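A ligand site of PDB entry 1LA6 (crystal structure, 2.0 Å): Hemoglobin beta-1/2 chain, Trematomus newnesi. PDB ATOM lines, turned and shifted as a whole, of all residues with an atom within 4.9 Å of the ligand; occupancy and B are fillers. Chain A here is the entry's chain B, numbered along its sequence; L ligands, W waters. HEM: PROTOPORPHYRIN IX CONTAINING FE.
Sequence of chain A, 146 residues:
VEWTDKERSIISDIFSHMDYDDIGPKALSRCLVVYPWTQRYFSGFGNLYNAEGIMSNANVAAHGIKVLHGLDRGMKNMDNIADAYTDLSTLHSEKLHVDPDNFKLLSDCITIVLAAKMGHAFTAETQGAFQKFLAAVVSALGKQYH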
ATOM      1  N   LEU A  32      16.962  10.034 -22.132  1.00  0.00           N
ATOM      2  CA  LEU A  32      17.035  10.121 -23.583  1.00  0.00           C
ATOM      3  C   LEU A  32      15.654  10.356 -24.201  1.00  0.00           C
ATOM      4  O   LEU A  32      15.545  10.876 -25.301  1.00  0.00           O
ATOM      5  CB  LEU A  32      17.679   8.859 -24.171  1.00  0.00           C
ATOM      6  CG  LEU A  32      19.084   8.516 -23.679  1.00  0.00           C
ATOM      7  CD1 LEU A  32      19.735   7.544 -24.647  1.00  0.00           C
ATOM      8  CD2 LEU A  32      19.932   9.750 -23.559  1.00  0.00           C
ATOM      9  N   THR A  38      20.019  14.450 -25.825  1.00  0.00           N
ATOM     10  CA  THR A  38      21.108  13.733 -25.187  1.00  0.00           C
ATOM     11  C   THR A  38      21.252  12.379 -25.880  1.00  0.00           C
ATOM     12  O   THR A  38      22.148  11.617 -25.550  1.00  0.00           O
ATOM     13  CB  THR A  38      20.865  13.505 -23.685  1.00  0.00           C
ATOM     14  OG1 THR A  38      19.587  12.875 -23.486  1.00  0.00           O
ATOM     15  CG2 THR A  38      20.900  14.817 -22.921  1.00  0.00           C
ATOM     16  N   TYR A  41      24.673  11.500 -27.933  1.00  0.00           N
ATOM     17  CA  TYR A  41      25.889  10.911 -27.376  1.00  0.00           C
ATOM     18  C   TYR A  41      25.922   9.397 -27.501  1.00  0.00           C
ATOM     19  O   TYR A  41      26.971   8.774 -27.301  1.00  0.00           O
ATOM     20  CB  TYR A  41      26.018  11.289 -25.900  1.00  0.00           C
ATOM     21  CG  TYR A  41      26.012  12.766 -25.687  1.00  0.00           C
ATOM     22  CD1 TYR A  41      24.885  13.425 -25.228  1.00  0.00           C
ATOM     23  CD2 TYR A  41      27.150  13.516 -25.955  1.00  0.00           C
ATOM     24  CE1 TYR A  41      24.893  14.775 -25.033  1.00  0.00           C
ATOM     25  CE2 TYR A  41      27.162  14.875 -25.764  1.00  0.00           C
ATOM     26  CZ  TYR A  41      26.033  15.502 -25.294  1.00  0.00           C
ATOM     27  OH  TYR A  41      26.061  16.853 -25.075  1.00  0.00           O
ATOM     28  N   PHE A  42      24.783   8.803 -27.838  1.00  0.00           N
ATOM     29  CA  PHE A  42      24.677   7.365 -27.994  1.00  0.00           C
ATOM     30  C   PHE A  42      24.335   6.955 -29.419  1.00  0.00           C
ATOM     31  O   PHE A  42      23.902   5.827 -29.667  1.00  0.00           O
ATOM     32  CB  PHE A  42      23.693   6.803 -26.963  1.00  0.00           C
ATOM     33  CG  PHE A  42      24.073   7.113 -25.549  1.00  0.00           C
ATOM     34  CD1 PHE A  42      24.931   6.273 -24.842  1.00  0.00           C
ATOM     35  CD2 PHE A  42      23.668   8.319 -24.955  1.00  0.00           C
ATOM     36  CE1 PHE A  42      25.386   6.619 -23.581  1.00  0.00           C
ATOM     37  CE2 PHE A  42      24.115   8.668 -23.700  1.00  0.00           C
ATOM     38  CZ  PHE A  42      24.974   7.831 -23.010  1.00  0.00           C
ATOM     39  N   HIS A  63      25.886   2.041 -20.036  1.00  0.00           N
ATOM     40  CA  HIS A  63      26.312   3.325 -19.506  1.00  0.00           C
ATOM     41  C   HIS A  63      25.459   3.740 -18.305  1.00  0.00           C
ATOM     42  O   HIS A  63      25.943   4.382 -17.387  1.00  0.00           O
ATOM     43  CB  HIS A  63      26.310   4.412 -20.579  1.00  0.00           C
ATOM     44  CG  HIS A  63      26.677   5.764 -20.054  1.00  0.00           C
ATOM     45  ND1 HIS A  63      25.766   6.679 -19.609  1.00  0.00           N
ATOM     46  CD2 HIS A  63      27.891   6.322 -19.840  1.00  0.00           C
ATOM     47  CE1 HIS A  63      26.431   7.746 -19.129  1.00  0.00           C
ATOM     48  NE2 HIS A  63      27.729   7.577 -19.250  1.00  0.00           N
ATOM     49  N   LYS A  66      26.986   2.139 -15.429  1.00  0.00           N
ATOM     50  CA  LYS A  66      28.240   2.836 -15.132  1.00  0.00           C
ATOM     51  C   LYS A  66      28.020   4.120 -14.359  1.00  0.00           C
ATOM     52  O   LYS A  66      28.828   4.482 -13.503  1.00  0.00           O
ATOM     53  CB  LYS A  66      28.993   3.155 -16.409  1.00  0.00           C
ATOM     54  CG  LYS A  66      29.465   1.964 -17.186  1.00  0.00           C
ATOM     55  CD  LYS A  66      30.392   2.450 -18.263  1.00  0.00           C
ATOM     56  CE  LYS A  66      30.825   1.338 -19.183  1.00  0.00           C
ATOM     57  NZ  LYS A  66      31.598   1.920 -20.317  1.00  0.00           N
ATOM     58  N   VAL A  67      26.952   4.856 -14.688  1.00  0.00           N
ATOM     59  CA  VAL A  67      26.645   6.098 -13.978  1.00  0.00           C
ATOM     60  C   VAL A  67      26.433   5.813 -12.482  1.00  0.00           C
ATOM     61  O   VAL A  67      27.027   6.471 -11.637  1.00  0.00           O
ATOM     62  CB  VAL A  67      25.380   6.789 -14.561  1.00  0.00           C
ATOM     63  CG1 VAL A  67      24.917   7.935 -13.658  1.00  0.00           C
ATOM     64  CG2 VAL A  67      25.670   7.315 -15.945  1.00  0.00           C
ATOM     65  N   GLY A  70      29.443   5.044 -10.817  1.00  0.00           N
ATOM     66  CA  GLY A  70      30.247   6.242 -10.667  1.00  0.00           C
ATOM     67  C   GLY A  70      29.802   7.009  -9.439  1.00  0.00           C
ATOM     68  O   GLY A  70      30.591   7.677  -8.794  1.00  0.00           O
ATOM     69  N   LEU A  71      28.509   6.937  -9.139  1.00  0.00           N
ATOM     70  CA  LEU A  71      27.947   7.627  -7.978  1.00  0.00           C
ATOM     71  C   LEU A  71      28.410   6.902  -6.712  1.00  0.00           C
ATOM     72  O   LEU A  71      28.709   7.521  -5.691  1.00  0.00           O
ATOM     73  CB  LEU A  71      26.409   7.616  -8.058  1.00  0.00           C
ATOM     74  CG  LEU A  71      25.767   8.510  -9.115  1.00  0.00           C
ATOM     75  CD1 LEU A  71      24.266   8.434  -8.994  1.00  0.00           C
ATOM     76  CD2 LEU A  71      26.250   9.910  -8.910  1.00  0.00           C
ATOM     77  N   TYR A  85      36.142  12.930  -8.916  1.00  0.00           N
ATOM     78  CA  TYR A  85      35.665  12.911 -10.294  1.00  0.00           C
ATOM     79  C   TYR A  85      36.539  13.555 -11.359  1.00  0.00           C
ATOM     80  O   TYR A  85      36.123  13.677 -12.514  1.00  0.00           O
ATOM     81  CB  TYR A  85      34.243  13.452 -10.345  1.00  0.00           C
ATOM     82  CG  TYR A  85      33.267  12.573  -9.623  1.00  0.00           C
ATOM     83  CD1 TYR A  85      32.855  12.872  -8.329  1.00  0.00           C
ATOM     84  CD2 TYR A  85      32.768  11.413 -10.210  1.00  0.00           C
ATOM     85  CE1 TYR A  85      31.972  12.042  -7.632  1.00  0.00           C
ATOM     86  CE2 TYR A  85      31.886  10.573  -9.533  1.00  0.00           C
ATOM     87  CZ  TYR A  85      31.496  10.895  -8.244  1.00  0.00           C
ATOM     88  OH  TYR A  85      30.610  10.092  -7.570  1.00  0.00           O
ATOM     89  N   LEU A  88      36.789  11.524 -14.659  1.00  0.00           N
ATOM     90  CA  LEU A  88      35.509  11.526 -15.370  1.00  0.00           C
ATOM     91  C   LEU A  88      35.077  12.905 -15.891  1.00  0.00           C
ATOM     92  O   LEU A  88      34.473  13.004 -16.973  1.00  0.00           O
ATOM     93  CB  LEU A  88      34.413  10.922 -14.486  1.00  0.00           C
ATOM     94  CG  LEU A  88      34.476   9.402 -14.320  1.00  0.00           C
ATOM     95  CD1 LEU A  88      33.308   8.932 -13.473  1.00  0.00           C
ATOM     96  CD2 LEU A  88      34.468   8.752 -15.676  1.00  0.00           C
ATOM     97  N   LEU A  91      37.042  13.337 -18.963  1.00  0.00           N
ATOM     98  CA  LEU A  91      36.607  12.422 -20.017  1.00  0.00           C
ATOM     99  C   LEU A  91      35.374  12.962 -20.730  1.00  0.00           C
ATOM    100  O   LEU A  91      35.389  13.193 -21.934  1.00  0.00           O
ATOM    101  CB  LEU A  91      36.272  11.033 -19.448  1.00  0.00           C
ATOM    102  CG  LEU A  91      35.870  10.042 -20.548  1.00  0.00           C
ATOM    103  CD1 LEU A  91      37.105   9.684 -21.350  1.00  0.00           C
ATOM    104  CD2 LEU A  91      35.231   8.792 -19.963  1.00  0.00           C
ATOM    105  N   HIS A  92      34.305  13.188 -19.962  1.00  0.00           N
ATOM    106  CA  HIS A  92      33.046  13.687 -20.503  1.00  0.00           C
ATOM    107  C   HIS A  92      33.172  15.041 -21.158  1.00  0.00           C
ATOM    108  O   HIS A  92      32.515  15.317 -22.158  1.00  0.00           O
ATOM    109  CB  HIS A  92      31.975  13.707 -19.405  1.00  0.00           C
ATOM    110  CG  HIS A  92      31.527  12.345 -18.997  1.00  0.00           C
ATOM    111  ND1 HIS A  92      32.148  11.582 -18.029  1.00  0.00           N
ATOM    112  CD2 HIS A  92      30.534  11.562 -19.491  1.00  0.00           C
ATOM    113  CE1 HIS A  92      31.523  10.394 -17.993  1.00  0.00           C
ATOM    114  NE2 HIS A  92      30.536  10.345 -18.866  1.00  0.00           N
ATOM    115  N   LYS A  95      36.997  14.732 -23.952  1.00  0.00           N
ATOM    116  CA  LYS A  95      36.833  13.664 -24.932  1.00  0.00           C
ATOM    117  C   LYS A  95      35.413  13.516 -25.468  1.00  0.00           C
ATOM    118  O   LYS A  95      35.203  13.534 -26.685  1.00  0.00           O
ATOM    119  CB  LYS A  95      37.321  12.329 -24.356  1.00  0.00           C
ATOM    120  CG  LYS A  95      37.131  11.130 -25.304  1.00  0.00           C
ATOM    121  CD  LYS A  95      37.062   9.802 -24.550  1.00  0.00           C
ATOM    122  CE  LYS A  95      36.372   8.699 -25.355  1.00  0.00           C
ATOM    123  NZ  LYS A  95      35.889   7.561 -24.495  1.00  0.00           N
ATOM    124  N   LEU A  96      34.443  13.375 -24.577  1.00  0.00           N
ATOM    125  CA  LEU A  96      33.043  13.179 -24.950  1.00  0.00           C
ATOM    126  C   LEU A  96      32.271  14.430 -25.379  1.00  0.00           C
ATOM    127  O   LEU A  96      31.314  14.331 -26.138  1.00  0.00           O
ATOM    128  CB  LEU A  96      32.307  12.451 -23.820  1.00  0.00           C
ATOM    129  CG  LEU A  96      32.372  10.916 -23.710  1.00  0.00           C
ATOM    130  CD1 LEU A  96      33.291  10.311 -24.764  1.00  0.00           C
ATOM    131  CD2 LEU A  96      32.784  10.501 -22.312  1.00  0.00           C
ATOM    132  N   VAL A  98      30.305  16.394 -23.636  1.00  0.00           N
ATOM    133  CA  VAL A  98      28.957  16.419 -23.107  1.00  0.00           C
ATOM    134  C   VAL A  98      28.702  17.813 -22.542  1.00  0.00           C
ATOM    135  O   VAL A  98      29.502  18.308 -21.725  1.00  0.00           O
ATOM    136  CB  VAL A  98      28.769  15.351 -21.981  1.00  0.00           C
ATOM    137  CG1 VAL A  98      27.416  15.549 -21.267  1.00  0.00           C
ATOM    138  CG2 VAL A  98      28.862  13.950 -22.569  1.00  0.00           C
ATOM    139  N   ASN A 102      23.567  18.902 -19.269  1.00  0.00           N
ATOM    140  CA  ASN A 102      23.024  17.544 -19.318  1.00  0.00           C
ATOM    141  C   ASN A 102      23.227  16.714 -18.057  1.00  0.00           C
ATOM    142  O   ASN A 102      22.529  15.714 -17.861  1.00  0.00           O
ATOM    143  CB  ASN A 102      23.563  16.826 -20.541  1.00  0.00           C
ATOM    144  CG  ASN A 102      23.268  17.570 -21.804  1.00  0.00           C
ATOM    145  OD1 ASN A 102      22.215  18.177 -21.937  1.00  0.00           O
ATOM    146  ND2 ASN A 102      24.220  17.587 -22.721  1.00  0.00           N
ATOM    147  N   PHE A 103      24.163  17.126 -17.205  1.00  0.00           N
ATOM    148  CA  PHE A 103      24.419  16.404 -15.968  1.00  0.00           C
ATOM    149  C   PHE A 103      23.257  16.629 -15.046  1.00  0.00           C
ATOM    150  O   PHE A 103      22.825  15.711 -14.343  1.00  0.00           O
ATOM    151  CB  PHE A 103      25.714  16.864 -15.304  1.00  0.00           C
ATOM    152  CG  PHE A 103      26.954  16.420 -16.019  1.00  0.00           C
ATOM    153  CD1 PHE A 103      27.081  15.097 -16.449  1.00  0.00           C
ATOM    154  CD2 PHE A 103      27.981  17.321 -16.304  1.00  0.00           C
ATOM    155  CE1 PHE A 103      28.219  14.670 -17.143  1.00  0.00           C
ATOM    156  CE2 PHE A 103      29.111  16.910 -17.000  1.00  0.00           C
ATOM    157  CZ  PHE A 103      29.229  15.571 -17.423  1.00  0.00           C
ATOM    158  N   LEU A 106      20.171  14.452 -16.307  1.00  0.00           N
ATOM    159  CA  LEU A 106      20.277  13.050 -15.883  1.00  0.00           C
ATOM    160  C   LEU A 106      19.983  12.919 -14.390  1.00  0.00           C
ATOM    161  O   LEU A 106      19.252  12.052 -13.966  1.00  0.00           O
ATOM    162  CB  LEU A 106      21.682  12.507 -16.208  1.00  0.00           C
ATOM    163  CG  LEU A 106      21.953  11.046 -15.848  1.00  0.00           C
ATOM    164  CD1 LEU A 106      20.859  10.142 -16.407  1.00  0.00           C
ATOM    165  CD2 LEU A 106      23.293  10.651 -16.414  1.00  0.00           C
ATOM    166  N   LEU A 141      31.584  17.133 -11.669  1.00  0.00           N
ATOM    167  CA  LEU A 141      31.684  16.743 -13.081  1.00  0.00           C
ATOM    168  C   LEU A 141      31.862  17.921 -14.032  1.00  0.00           C
ATOM    169  O   LEU A 141      32.454  17.784 -15.103  1.00  0.00           O
ATOM    170  CB  LEU A 141      30.490  15.899 -13.494  1.00  0.00           C
ATOM    171  CG  LEU A 141      30.541  14.421 -13.085  1.00  0.00           C
ATOM    172  CD1 LEU A 141      29.267  13.767 -13.528  1.00  0.00           C
ATOM    173  CD2 LEU A 141      31.713  13.723 -13.712  1.00  0.00           C
HETATM  174  CHA HEM L   1      31.246   7.126 -20.353  1.00  0.00           C
HETATM  175  CHB HEM L   1      29.983   8.030 -15.733  1.00  0.00           C
HETATM  176  CHC HEM L   1      27.104  11.544 -17.313  1.00  0.00           C
HETATM  177  CHD HEM L   1      27.742  10.151 -21.929  1.00  0.00           C
HETATM  178  C1A HEM L   1      31.167   7.049 -18.941  1.00  0.00           C
HETATM  179  C2A HEM L   1      31.879   6.105 -18.072  1.00  0.00           C
HETATM  180  C3A HEM L   1      31.508   6.336 -16.798  1.00  0.00           C
HETATM  181  C4A HEM L   1      30.548   7.422 -16.844  1.00  0.00           C
HETATM  182  CMA HEM L   1      31.943   5.525 -15.567  1.00  0.00           C
HETATM  183  CAA HEM L   1      32.827   5.028 -18.507  1.00  0.00           C
HETATM  184  CBA HEM L   1      34.163   5.662 -18.816  1.00  0.00           C
HETATM  185  CGA HEM L   1      35.222   4.636 -19.083  1.00  0.00           C
HETATM  186  O1A HEM L   1      36.225   4.602 -18.319  1.00  0.00           O
HETATM  187  O2A HEM L   1      35.073   3.858 -20.057  1.00  0.00           O
HETATM  188  C1B HEM L   1      29.100   9.092 -15.768  1.00  0.00           C
HETATM  189  C2B HEM L   1      28.634   9.771 -14.569  1.00  0.00           C
HETATM  190  C3B HEM L   1      27.785  10.738 -14.989  1.00  0.00           C
HETATM  191  C4B HEM L   1      27.829  10.711 -16.481  1.00  0.00           C
HETATM  192  CMB HEM L   1      28.988   9.484 -13.095  1.00  0.00           C
HETATM  193  CAB HEM L   1      26.884  11.277 -14.057  1.00  0.00           C
HETATM  194  CBB HEM L   1      26.024  12.485 -14.067  1.00  0.00           C
HETATM  195  C1C HEM L   1      26.958  11.486 -18.700  1.00  0.00           C
HETATM  196  C2C HEM L   1      26.020  12.306 -19.524  1.00  0.00           C
HETATM  197  C3C HEM L   1      26.156  11.846 -20.801  1.00  0.00           C
HETATM  198  C4C HEM L   1      27.172  10.779 -20.808  1.00  0.00           C
HETATM  199  CMC HEM L   1      25.037  13.409 -19.102  1.00  0.00           C
HETATM  200  CAC HEM L   1      25.440  12.299 -21.893  1.00  0.00           C
HETATM  201  CBC HEM L   1      24.194  11.663 -22.235  1.00  0.00           C
HETATM  202  C1D HEM L   1      28.817   9.222 -21.909  1.00  0.00           C
HETATM  203  C2D HEM L   1      29.334   8.528 -23.080  1.00  0.00           C
HETATM  204  C3D HEM L   1      30.372   7.755 -22.655  1.00  0.00           C
HETATM  205  C4D HEM L   1      30.435   7.900 -21.205  1.00  0.00           C
HETATM  206  CMD HEM L   1      28.778   8.635 -24.521  1.00  0.00           C
HETATM  207  CAD HEM L   1      31.372   7.012 -23.535  1.00  0.00           C
HETATM  208  CBD HEM L   1      30.934   5.648 -24.038  1.00  0.00           C
HETATM  209  CGD HEM L   1      30.764   4.626 -22.923  1.00  0.00           C
HETATM  210  O1D HEM L   1      31.785   4.058 -22.473  1.00  0.00           O
HETATM  211  O2D HEM L   1      29.611   4.384 -22.502  1.00  0.00           O
HETATM  212  NA  HEM L   1      30.301   7.812 -18.180  1.00  0.00           N
HETATM  213  NB  HEM L   1      28.583   9.660 -16.957  1.00  0.00           N
HETATM  214  NC  HEM L   1      27.633  10.530 -19.496  1.00  0.00           N
HETATM  215  ND  HEM L   1      29.466   8.772 -20.762  1.00  0.00           N
HETATM  216 FE   HEM L   1      28.965   9.102 -18.911  1.00  0.00          FE
HETATM  217  O   HOH W   1      27.784   2.383 -22.796  1.00  0.00           O
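Water W1 bridges an oxygen (O2D) of the ligand and the backbone NH (N) of His 63.
NE2 of His 63 binds FE of the ligand, at 2.0 Å. A ring nitrogen (NE2) of His 92 binds an iron atom (FE) of the ligand, 2.0 Å away. NZ of Lys 66 is in salt-bridge range of O1D of the ligand, 3.0 Å away.
Thr 38 touches the ligand (O to CBC, 3.9 Å). Tyr 41 touches the ligand (O to CMD, 3.3 Å). Phe 42 touches the ligand (CE2 to CBC, 3.3 Å). Val 67 touches the ligand (CG2 to C1B, 3.9 Å). CD2 of Leu 88 touches C3A of the ligand (3.98 Å). CD2 of Leu 91 touches CBA of the ligand, 3.5 Å away. Leu 96 touches the ligand. Val 98 touches the ligand (CG1 to CAC, 3.9 Å). Asn 102 touches the ligand (O to CMC, 3.6 Å). Phe 103 touches the ligand (CE1 to CHC, 3.3 Å). Leu 141 touches the ligand. Hydrophobic or aromatic side chains within 4 Å of the ligand: Tyr 41, Phe 42, His 63, Val 67, Leu 88, Leu 91, His 92, Leu 96, Val 98, Phe 103 and Leu 141.
The backbone carbonyl oxygen (O) of His 92 sits at hydrogen-bond distance from the backbone NH (N) of Val 98, 2.9 Å away. A ring nitrogen (ND1) of His 92 is in hydrogen-bond range of the backbone carbonyl oxygen (O) of Leu 88 (2.9 Å). OH of Tyr 41 lies within hydrogen-bond range of ND2 of Asn 102, at 3.1 Å. The backbone NH of Leu 96 sits at hydrogen-bond distance from the backbone carbonyl oxygen of Leu 91, 2.8 Å away.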
